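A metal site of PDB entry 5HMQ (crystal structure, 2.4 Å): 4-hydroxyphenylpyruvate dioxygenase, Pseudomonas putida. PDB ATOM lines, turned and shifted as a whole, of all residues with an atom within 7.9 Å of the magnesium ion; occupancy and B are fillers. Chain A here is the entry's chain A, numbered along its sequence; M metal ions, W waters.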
ATOM      1  N   GLU A  32     -16.411 -15.016 -27.255  1.00  0.00           N
ATOM      2  CA  GLU A  32     -16.389 -16.194 -28.113  1.00  0.00           C
ATOM      3  C   GLU A  32     -17.521 -17.119 -27.674  1.00  0.00           C
ATOM      4  O   GLU A  32     -17.582 -17.514 -26.508  1.00  0.00           O
ATOM      5  CB  GLU A  32     -15.045 -16.922 -28.038  1.00  0.00           C
ATOM      6  CG  GLU A  32     -13.842 -16.046 -27.747  1.00  0.00           C
ATOM      7  CD  GLU A  32     -12.572 -16.861 -27.615  1.00  0.00           C
ATOM      8  OE1 GLU A  32     -12.569 -18.034 -28.051  1.00  0.00           O
ATOM      9  OE2 GLU A  32     -11.584 -16.334 -27.065  1.00  0.00           O
ATOM     10  N   LEU A  61     -16.240 -14.358 -32.161  1.00  0.00           N
ATOM     11  CA  LEU A  61     -15.748 -15.652 -32.630  1.00  0.00           C
ATOM     12  C   LEU A  61     -16.768 -16.730 -32.315  1.00  0.00           C
ATOM     13  O   LEU A  61     -17.433 -16.675 -31.275  1.00  0.00           O
ATOM     14  CB  LEU A  61     -14.401 -15.990 -31.984  1.00  0.00           C
ATOM     15  CG  LEU A  61     -13.784 -17.358 -32.249  1.00  0.00           C
ATOM     16  CD1 LEU A  61     -13.353 -17.483 -33.698  1.00  0.00           C
ATOM     17  CD2 LEU A  61     -12.599 -17.599 -31.331  1.00  0.00           C
ATOM     18  N   GLN A  63     -16.791 -20.973 -32.038  1.00  0.00           N
ATOM     19  CA  GLN A  63     -15.822 -22.063 -31.884  1.00  0.00           C
ATOM     20  C   GLN A  63     -16.417 -23.205 -31.054  1.00  0.00           C
ATOM     21  O   GLN A  63     -17.342 -22.991 -30.268  1.00  0.00           O
ATOM     22  CB  GLN A  63     -14.521 -21.529 -31.264  1.00  0.00           C
ATOM     23  CG  GLN A  63     -14.660 -20.986 -29.852  1.00  0.00           C
ATOM     24  CD  GLN A  63     -13.727 -21.671 -28.878  1.00  0.00           C
ATOM     25  OE1 GLN A  63     -13.543 -22.882 -28.938  1.00  0.00           O
ATOM     26  NE2 GLN A  63     -13.123 -20.892 -27.988  1.00  0.00           N
ATOM     27  N   LEU A  99     -13.325 -20.600 -35.451  1.00  0.00           N
ATOM     28  CA  LEU A  99     -12.035 -21.197 -35.153  1.00  0.00           C
ATOM     29  C   LEU A  99     -12.027 -22.652 -35.609  1.00  0.00           C
ATOM     30  O   LEU A  99     -12.885 -23.438 -35.208  1.00  0.00           O
ATOM     31  CB  LEU A  99     -11.730 -21.093 -33.658  1.00  0.00           C
ATOM     32  CG  LEU A  99     -10.389 -21.569 -33.088  1.00  0.00           C
ATOM     33  CD1 LEU A  99     -10.047 -20.784 -31.839  1.00  0.00           C
ATOM     34  CD2 LEU A  99     -10.407 -23.062 -32.776  1.00  0.00           C
ATOM     35  N   CYS A 101      -9.582 -25.797 -35.343  1.00  0.00           N
ATOM     36  CA  CYS A 101      -8.393 -26.306 -34.682  1.00  0.00           C
ATOM     37  C   CYS A 101      -7.856 -27.543 -35.410  1.00  0.00           C
ATOM     38  O   CYS A 101      -8.607 -28.312 -36.001  1.00  0.00           O
ATOM     39  CB  CYS A 101      -8.689 -26.627 -33.204  1.00  0.00           C
ATOM     40  SG  CYS A 101     -10.200 -27.547 -32.865  1.00  0.00           S
ATOM     41  N   GLU A 136      -6.192 -22.721 -35.961  1.00  0.00           N
ATOM     42  CA  GLU A 136      -5.454 -22.808 -34.703  1.00  0.00           C
ATOM     43  C   GLU A 136      -4.792 -24.176 -34.598  1.00  0.00           C
ATOM     44  O   GLU A 136      -5.422 -25.198 -34.868  1.00  0.00           O
ATOM     45  CB  GLU A 136      -6.379 -22.593 -33.507  1.00  0.00           C
ATOM     46  CG  GLU A 136      -5.702 -22.762 -32.153  1.00  0.00           C
ATOM     47  CD  GLU A 136      -6.697 -22.996 -31.025  1.00  0.00           C
ATOM     48  OE1 GLU A 136      -7.523 -23.923 -31.145  1.00  0.00           O
ATOM     49  OE2 GLU A 136      -6.636 -22.254 -30.023  1.00  0.00           O
ATOM     50  N   ALA A 137      -3.520 -24.183 -34.210  1.00  0.00           N
ATOM     51  CA  ALA A 137      -2.795 -25.421 -33.954  1.00  0.00           C
ATOM     52  C   ALA A 137      -3.015 -25.854 -32.506  1.00  0.00           C
ATOM     53  O   ALA A 137      -2.691 -25.107 -31.582  1.00  0.00           O
ATOM     54  CB  ALA A 137      -1.314 -25.260 -34.237  1.00  0.00           C
ATOM     55  N   LEU A 138      -3.549 -27.055 -32.319  1.00  0.00           N
ATOM     56  CA  LEU A 138      -3.555 -27.676 -31.005  1.00  0.00           C
ATOM     57  C   LEU A 138      -2.184 -28.265 -30.715  1.00  0.00           C
ATOM     58  O   LEU A 138      -1.553 -28.860 -31.593  1.00  0.00           O
ATOM     59  CB  LEU A 138      -4.628 -28.772 -30.909  1.00  0.00           C
ATOM     60  CG  LEU A 138      -6.073 -28.340 -31.164  1.00  0.00           C
ATOM     61  CD1 LEU A 138      -7.018 -29.537 -31.105  1.00  0.00           C
ATOM     62  CD2 LEU A 138      -6.502 -27.267 -30.167  1.00  0.00           C
ATOM     63  N   ILE A 165      -4.911 -18.142 -36.105  1.00  0.00           N
ATOM     64  CA  ILE A 165      -5.349 -17.898 -34.738  1.00  0.00           C
ATOM     65  C   ILE A 165      -4.252 -18.382 -33.809  1.00  0.00           C
ATOM     66  O   ILE A 165      -3.769 -19.514 -33.946  1.00  0.00           O
ATOM     67  CB  ILE A 165      -6.702 -18.570 -34.428  1.00  0.00           C
ATOM     68  CG1 ILE A 165      -7.832 -17.832 -35.153  1.00  0.00           C
ATOM     69  CG2 ILE A 165      -6.952 -18.590 -32.924  1.00  0.00           C
ATOM     70  CD1 ILE A 165      -9.224 -18.238 -34.707  1.00  0.00           C
ATOM     71  N   LEU A 166      -3.855 -17.523 -32.874  1.00  0.00           N
ATOM     72  CA  LEU A 166      -2.774 -17.802 -31.944  1.00  0.00           C
ATOM     73  C   LEU A 166      -3.340 -18.047 -30.555  1.00  0.00           C
ATOM     74  O   LEU A 166      -4.241 -17.332 -30.105  1.00  0.00           O
ATOM     75  CB  LEU A 166      -1.769 -16.648 -31.918  1.00  0.00           C
ATOM     76  CG  LEU A 166      -1.080 -16.348 -33.246  1.00  0.00           C
ATOM     77  CD1 LEU A 166      -0.294 -15.051 -33.176  1.00  0.00           C
ATOM     78  CD2 LEU A 166      -0.180 -17.507 -33.639  1.00  0.00           C
ATOM     79  N   ASP A 167      -2.802 -19.057 -29.872  1.00  0.00           N
ATOM     80  CA  ASP A 167      -3.224 -19.443 -28.538  1.00  0.00           C
ATOM     81  C   ASP A 167      -1.978 -19.568 -27.684  1.00  0.00           C
ATOM     82  O   ASP A 167      -1.107 -20.402 -27.977  1.00  0.00           O
ATOM     83  CB  ASP A 167      -4.018 -20.765 -28.565  1.00  0.00           C
ATOM     84  CG  ASP A 167      -4.552 -21.169 -27.197  1.00  0.00           C
ATOM     85  OD1 ASP A 167      -3.784 -21.157 -26.204  1.00  0.00           O
ATOM     86  OD2 ASP A 167      -5.744 -21.520 -27.116  1.00  0.00           O
ATOM     87  N   SER A 168      -1.874 -18.740 -26.647  1.00  0.00           N
ATOM     88  CA  SER A 168      -0.640 -18.676 -25.870  1.00  0.00           C
ATOM     89  C   SER A 168      -0.302 -20.007 -25.217  1.00  0.00           C
ATOM     90  O   SER A 168       0.870 -20.360 -25.094  1.00  0.00           O
ATOM     91  CB  SER A 168      -0.728 -17.580 -24.815  1.00  0.00           C
ATOM     92  OG  SER A 168      -1.764 -17.854 -23.887  1.00  0.00           O
ATOM     93  N   PHE A 169      -1.320 -20.779 -24.805  1.00  0.00           N
ATOM     94  CA  PHE A 169      -1.031 -22.056 -24.161  1.00  0.00           C
ATOM     95  C   PHE A 169      -0.457 -23.060 -25.156  1.00  0.00           C
ATOM     96  O   PHE A 169       0.509 -23.761 -24.860  1.00  0.00           O
ATOM     97  CB  PHE A 169      -2.264 -22.635 -23.484  1.00  0.00           C
ATOM     98  CG  PHE A 169      -2.003 -23.933 -22.786  1.00  0.00           C
ATOM     99  CD1 PHE A 169      -2.043 -25.135 -23.475  1.00  0.00           C
ATOM    100  CD2 PHE A 169      -1.679 -23.960 -21.439  1.00  0.00           C
ATOM    101  CE1 PHE A 169      -1.759 -26.326 -22.850  1.00  0.00           C
ATOM    102  CE2 PHE A 169      -1.408 -25.153 -20.799  1.00  0.00           C
ATOM    103  CZ  PHE A 169      -1.453 -26.340 -21.503  1.00  0.00           C
ATOM    104  N   HIS A 170      -1.083 -23.175 -26.333  1.00  0.00           N
ATOM    105  CA  HIS A 170      -0.634 -24.169 -27.302  1.00  0.00           C
ATOM    106  C   HIS A 170       0.810 -23.930 -27.738  1.00  0.00           C
ATOM    107  O   HIS A 170       1.524 -24.874 -28.062  1.00  0.00           O
ATOM    108  CB  HIS A 170      -1.567 -24.180 -28.516  1.00  0.00           C
ATOM    109  CG  HIS A 170      -2.919 -24.750 -28.231  1.00  0.00           C
ATOM    110  ND1 HIS A 170      -3.102 -26.015 -27.712  1.00  0.00           N
ATOM    111  CD2 HIS A 170      -4.157 -24.235 -28.402  1.00  0.00           C
ATOM    112  CE1 HIS A 170      -4.396 -26.244 -27.569  1.00  0.00           C
ATOM    113  NE2 HIS A 170      -5.053 -25.182 -27.975  1.00  0.00           N
ATOM    114  N   PHE A 191      -7.129 -13.795 -34.794  1.00  0.00           N
ATOM    115  CA  PHE A 191      -7.607 -13.883 -33.415  1.00  0.00           C
ATOM    116  C   PHE A 191      -6.466 -14.312 -32.506  1.00  0.00           C
ATOM    117  O   PHE A 191      -5.599 -15.089 -32.914  1.00  0.00           O
ATOM    118  CB  PHE A 191      -8.782 -14.874 -33.313  1.00  0.00           C
ATOM    119  CG  PHE A 191      -9.746 -14.557 -32.203  1.00  0.00           C
ATOM    120  CD1 PHE A 191     -10.757 -13.639 -32.389  1.00  0.00           C
ATOM    121  CD2 PHE A 191      -9.664 -15.221 -30.990  1.00  0.00           C
ATOM    122  CE1 PHE A 191     -11.652 -13.360 -31.371  1.00  0.00           C
ATOM    123  CE2 PHE A 191     -10.553 -14.941 -29.979  1.00  0.00           C
ATOM    124  CZ  PHE A 191     -11.552 -14.014 -30.168  1.00  0.00           C
ATOM    125  N   VAL A 192      -6.490 -13.812 -31.279  1.00  0.00           N
ATOM    126  CA  VAL A 192      -5.472 -14.115 -30.274  1.00  0.00           C
ATOM    127  C   VAL A 192      -6.179 -14.514 -28.987  1.00  0.00           C
ATOM    128  O   VAL A 192      -6.983 -13.734 -28.445  1.00  0.00           O
ATOM    129  CB  VAL A 192      -4.533 -12.925 -30.021  1.00  0.00           C
ATOM    130  CG1 VAL A 192      -3.595 -13.231 -28.859  1.00  0.00           C
ATOM    131  CG2 VAL A 192      -3.749 -12.586 -31.276  1.00  0.00           C
ATOM    132  N   GLN A 193      -5.888 -15.718 -28.490  1.00  0.00           N
ATOM    133  CA  GLN A 193      -6.434 -16.201 -27.236  1.00  0.00           C
ATOM    134  C   GLN A 193      -5.318 -16.228 -26.201  1.00  0.00           C
ATOM    135  O   GLN A 193      -4.272 -16.853 -26.422  1.00  0.00           O
ATOM    136  CB  GLN A 193      -7.029 -17.604 -27.395  1.00  0.00           C
ATOM    137  CG  GLN A 193      -8.111 -17.701 -28.443  1.00  0.00           C
ATOM    138  CD  GLN A 193      -8.642 -19.114 -28.589  1.00  0.00           C
ATOM    139  OE1 GLN A 193      -7.981 -19.983 -29.146  1.00  0.00           O
ATOM    140  NE2 GLN A 193      -9.869 -19.330 -28.134  1.00  0.00           N
ATOM    141  N   MET A 194      -5.531 -15.551 -25.086  1.00  0.00           N
ATOM    142  CA  MET A 194      -4.548 -15.563 -24.005  1.00  0.00           C
ATOM    143  C   MET A 194      -4.958 -16.543 -22.927  1.00  0.00           C
ATOM    144  O   MET A 194      -6.109 -16.532 -22.470  1.00  0.00           O
ATOM    145  CB  MET A 194      -4.368 -14.158 -23.420  1.00  0.00           C
ATOM    146  CG  MET A 194      -3.887 -13.129 -24.418  1.00  0.00           C
ATOM    147  SD  MET A 194      -2.227 -13.639 -25.301  1.00  0.00           S
ATOM    148  CE  MET A 194      -1.083 -13.799 -23.731  1.00  0.00           C
ATOM    149  N   ALA A 195      -4.030 -17.410 -22.539  1.00  0.00           N
ATOM    150  CA  ALA A 195      -4.289 -18.402 -21.506  1.00  0.00           C
ATOM    151  C   ALA A 195      -2.984 -18.685 -20.781  1.00  0.00           C
ATOM    152  O   ALA A 195      -1.984 -19.025 -21.400  1.00  0.00           O
ATOM    153  CB  ALA A 195      -4.848 -19.695 -22.109  1.00  0.00           C
ATOM    154  N   SER A 208      -3.845 -28.779 -20.696  1.00  0.00           N
ATOM    155  CA  SER A 208      -4.704 -27.708 -21.181  1.00  0.00           C
ATOM    156  C   SER A 208      -6.117 -27.831 -20.623  1.00  0.00           C
ATOM    157  O   SER A 208      -6.776 -26.814 -20.374  1.00  0.00           O
ATOM    158  CB  SER A 208      -4.751 -27.724 -22.708  1.00  0.00           C
ATOM    159  OG  SER A 208      -5.642 -26.747 -23.208  1.00  0.00           O
ATOM    160  N   ARG A 212      -5.496 -24.399 -17.249  1.00  0.00           N
ATOM    161  CA  ARG A 212      -5.477 -23.059 -17.819  1.00  0.00           C
ATOM    162  C   ARG A 212      -6.030 -22.055 -16.806  1.00  0.00           C
ATOM    163  O   ARG A 212      -6.959 -22.358 -16.055  1.00  0.00           O
ATOM    164  CB  ARG A 212      -6.303 -23.006 -19.104  1.00  0.00           C
ATOM    165  CG  ARG A 212      -5.555 -23.453 -20.338  1.00  0.00           C
ATOM    166  CD  ARG A 212      -6.436 -23.303 -21.552  1.00  0.00           C
ATOM    167  NE  ARG A 212      -5.865 -23.909 -22.748  1.00  0.00           N
ATOM    168  CZ  ARG A 212      -5.927 -23.358 -23.959  1.00  0.00           C
ATOM    169  NH1 ARG A 212      -6.534 -22.195 -24.123  1.00  0.00           N
ATOM    170  NH2 ARG A 212      -5.372 -23.969 -24.997  1.00  0.00           N
ATOM    171  N   LEU A 240      -9.583 -14.405 -24.090  1.00  0.00           N
ATOM    172  CA  LEU A 240      -9.216 -15.300 -22.996  1.00  0.00           C
ATOM    173  C   LEU A 240      -9.890 -16.641 -23.227  1.00  0.00           C
ATOM    174  O   LEU A 240     -11.084 -16.698 -23.519  1.00  0.00           O
ATOM    175  CB  LEU A 240      -9.665 -14.729 -21.647  1.00  0.00           C
ATOM    176  CG  LEU A 240      -9.056 -13.399 -21.221  1.00  0.00           C
ATOM    177  CD1 LEU A 240      -9.870 -12.794 -20.089  1.00  0.00           C
ATOM    178  CD2 LEU A 240      -7.617 -13.602 -20.794  1.00  0.00           C
ATOM    179  N   GLU A 241      -9.124 -17.725 -23.088  1.00  0.00           N
ATOM    180  CA  GLU A 241      -9.697 -19.072 -23.207  1.00  0.00           C
ATOM    181  C   GLU A 241      -9.102 -19.970 -22.129  1.00  0.00           C
ATOM    182  O   GLU A 241      -7.985 -20.473 -22.272  1.00  0.00           O
ATOM    183  CB  GLU A 241      -9.458 -19.650 -24.605  1.00  0.00           C
ATOM    184  CG  GLU A 241     -10.197 -20.945 -24.859  1.00  0.00           C
ATOM    185  CD  GLU A 241      -9.759 -21.636 -26.128  1.00  0.00           C
ATOM    186  OE1 GLU A 241      -8.563 -21.551 -26.467  1.00  0.00           O
ATOM    187  OE2 GLU A 241     -10.605 -22.272 -26.796  1.00  0.00           O
ATOM    188  N   ILE A 242      -9.866 -20.181 -21.052  1.00  0.00           N
ATOM    189  CA  ILE A 242      -9.571 -21.185 -20.034  1.00  0.00           C
ATOM    190  C   ILE A 242     -10.766 -22.131 -19.996  1.00  0.00           C
ATOM    191  O   ILE A 242     -11.876 -21.775 -20.398  1.00  0.00           O
ATOM    192  CB  ILE A 242      -9.305 -20.572 -18.648  1.00  0.00           C
ATOM    193  CG1 ILE A 242     -10.588 -19.976 -18.066  1.00  0.00           C
ATOM    194  CG2 ILE A 242      -8.236 -19.497 -18.750  1.00  0.00           C
ATOM    195  CD1 ILE A 242     -10.428 -19.466 -16.653  1.00  0.00           C
ATOM    196  N   PHE A 243     -10.526 -23.364 -19.547  1.00  0.00           N
ATOM    197  CA  PHE A 243     -11.580 -24.379 -19.584  1.00  0.00           C
ATOM    198  C   PHE A 243     -12.146 -24.687 -18.204  1.00  0.00           C
ATOM    199  O   PHE A 243     -11.546 -25.422 -17.417  1.00  0.00           O
ATOM    200  CB  PHE A 243     -11.063 -25.649 -20.267  1.00  0.00           C
ATOM    201  CG  PHE A 243     -10.687 -25.438 -21.704  1.00  0.00           C
ATOM    202  CD1 PHE A 243     -11.668 -25.242 -22.652  1.00  0.00           C
ATOM    203  CD2 PHE A 243      -9.353 -25.425 -22.094  1.00  0.00           C
ATOM    204  CE1 PHE A 243     -11.337 -25.035 -23.984  1.00  0.00           C
ATOM    205  CE2 PHE A 243      -9.016 -25.224 -23.421  1.00  0.00           C
ATOM    206  CZ  PHE A 243     -10.014 -25.029 -24.370  1.00  0.00           C
HETATM  207 MG    MG M   1      -7.472 -21.866 -28.210  1.00  0.00          MG
HETATM  208  O   HOH W   1      -9.537 -22.689 -29.181  1.00  0.00           O
HETATM  209  O   HOH W   2      -7.619 -24.421 -28.247  1.00  0.00           O
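Water W1 lies within hydrogen-bond range of OE2 of Glu 241 (2.6 Å) and OE1 of Glu 136 (3.1 Å). Water W2 lies within hydrogen-bond range of NE2 of His 170 (2.7 Å) and OE1 of Glu 136 (2.9 Å).
Of the 25 residues printed, 4 come within 4 Å of the magnesium ion.
The magnesium ion is bound by the side-chain carboxylate (OE2) of Glu 136, 2.0 Å away. OD2 of Asp 167 is bound to the magnesium ion (2.1 Å). The magnesium ion is bound by OE1 of Glu 241 (2.1 Å). OE1 of Gln 193 is bound to the magnesium ion. The magnesium ion is bound by water W1 (2.4 Å). Water W2 binds the magnesium ion.
The side-chain carboxylate (OD1) of Asp 167 is in hydrogen-bond range of the backbone NH (N) of His 170 (3.4 Å). The guanidinium group of Arg 212 is in salt-bridge range of the side-chain carboxylate of Asp 167 (3.4 Å). The backbone NH of Phe 169 sits at hydrogen-bond distance from the side-chain carboxylate of Asp 167 (2.9 Å). The backbone carbonyl oxygen of Glu 241 sits at hydrogen-bond distance from the guanidinium group of Arg 212 (2.9 Å). OE2 of Glu 241 is in hydrogen-bond range of NE2 of Gln 63 (3.1 Å). N of Gln 193 is in hydrogen-bond range of O of Leu 166, 2.8 Å away. The side-chain amide nitrogen (NE2) of Gln 193 lies within hydrogen-bond range of the side-chain carboxylate (OE1) of Glu 32 (3.0 Å). The backbone NH (N) of Ser 168 is in hydrogen-bond range of the backbone carbonyl oxygen (O) of Gln 193, 3.1 Å away.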
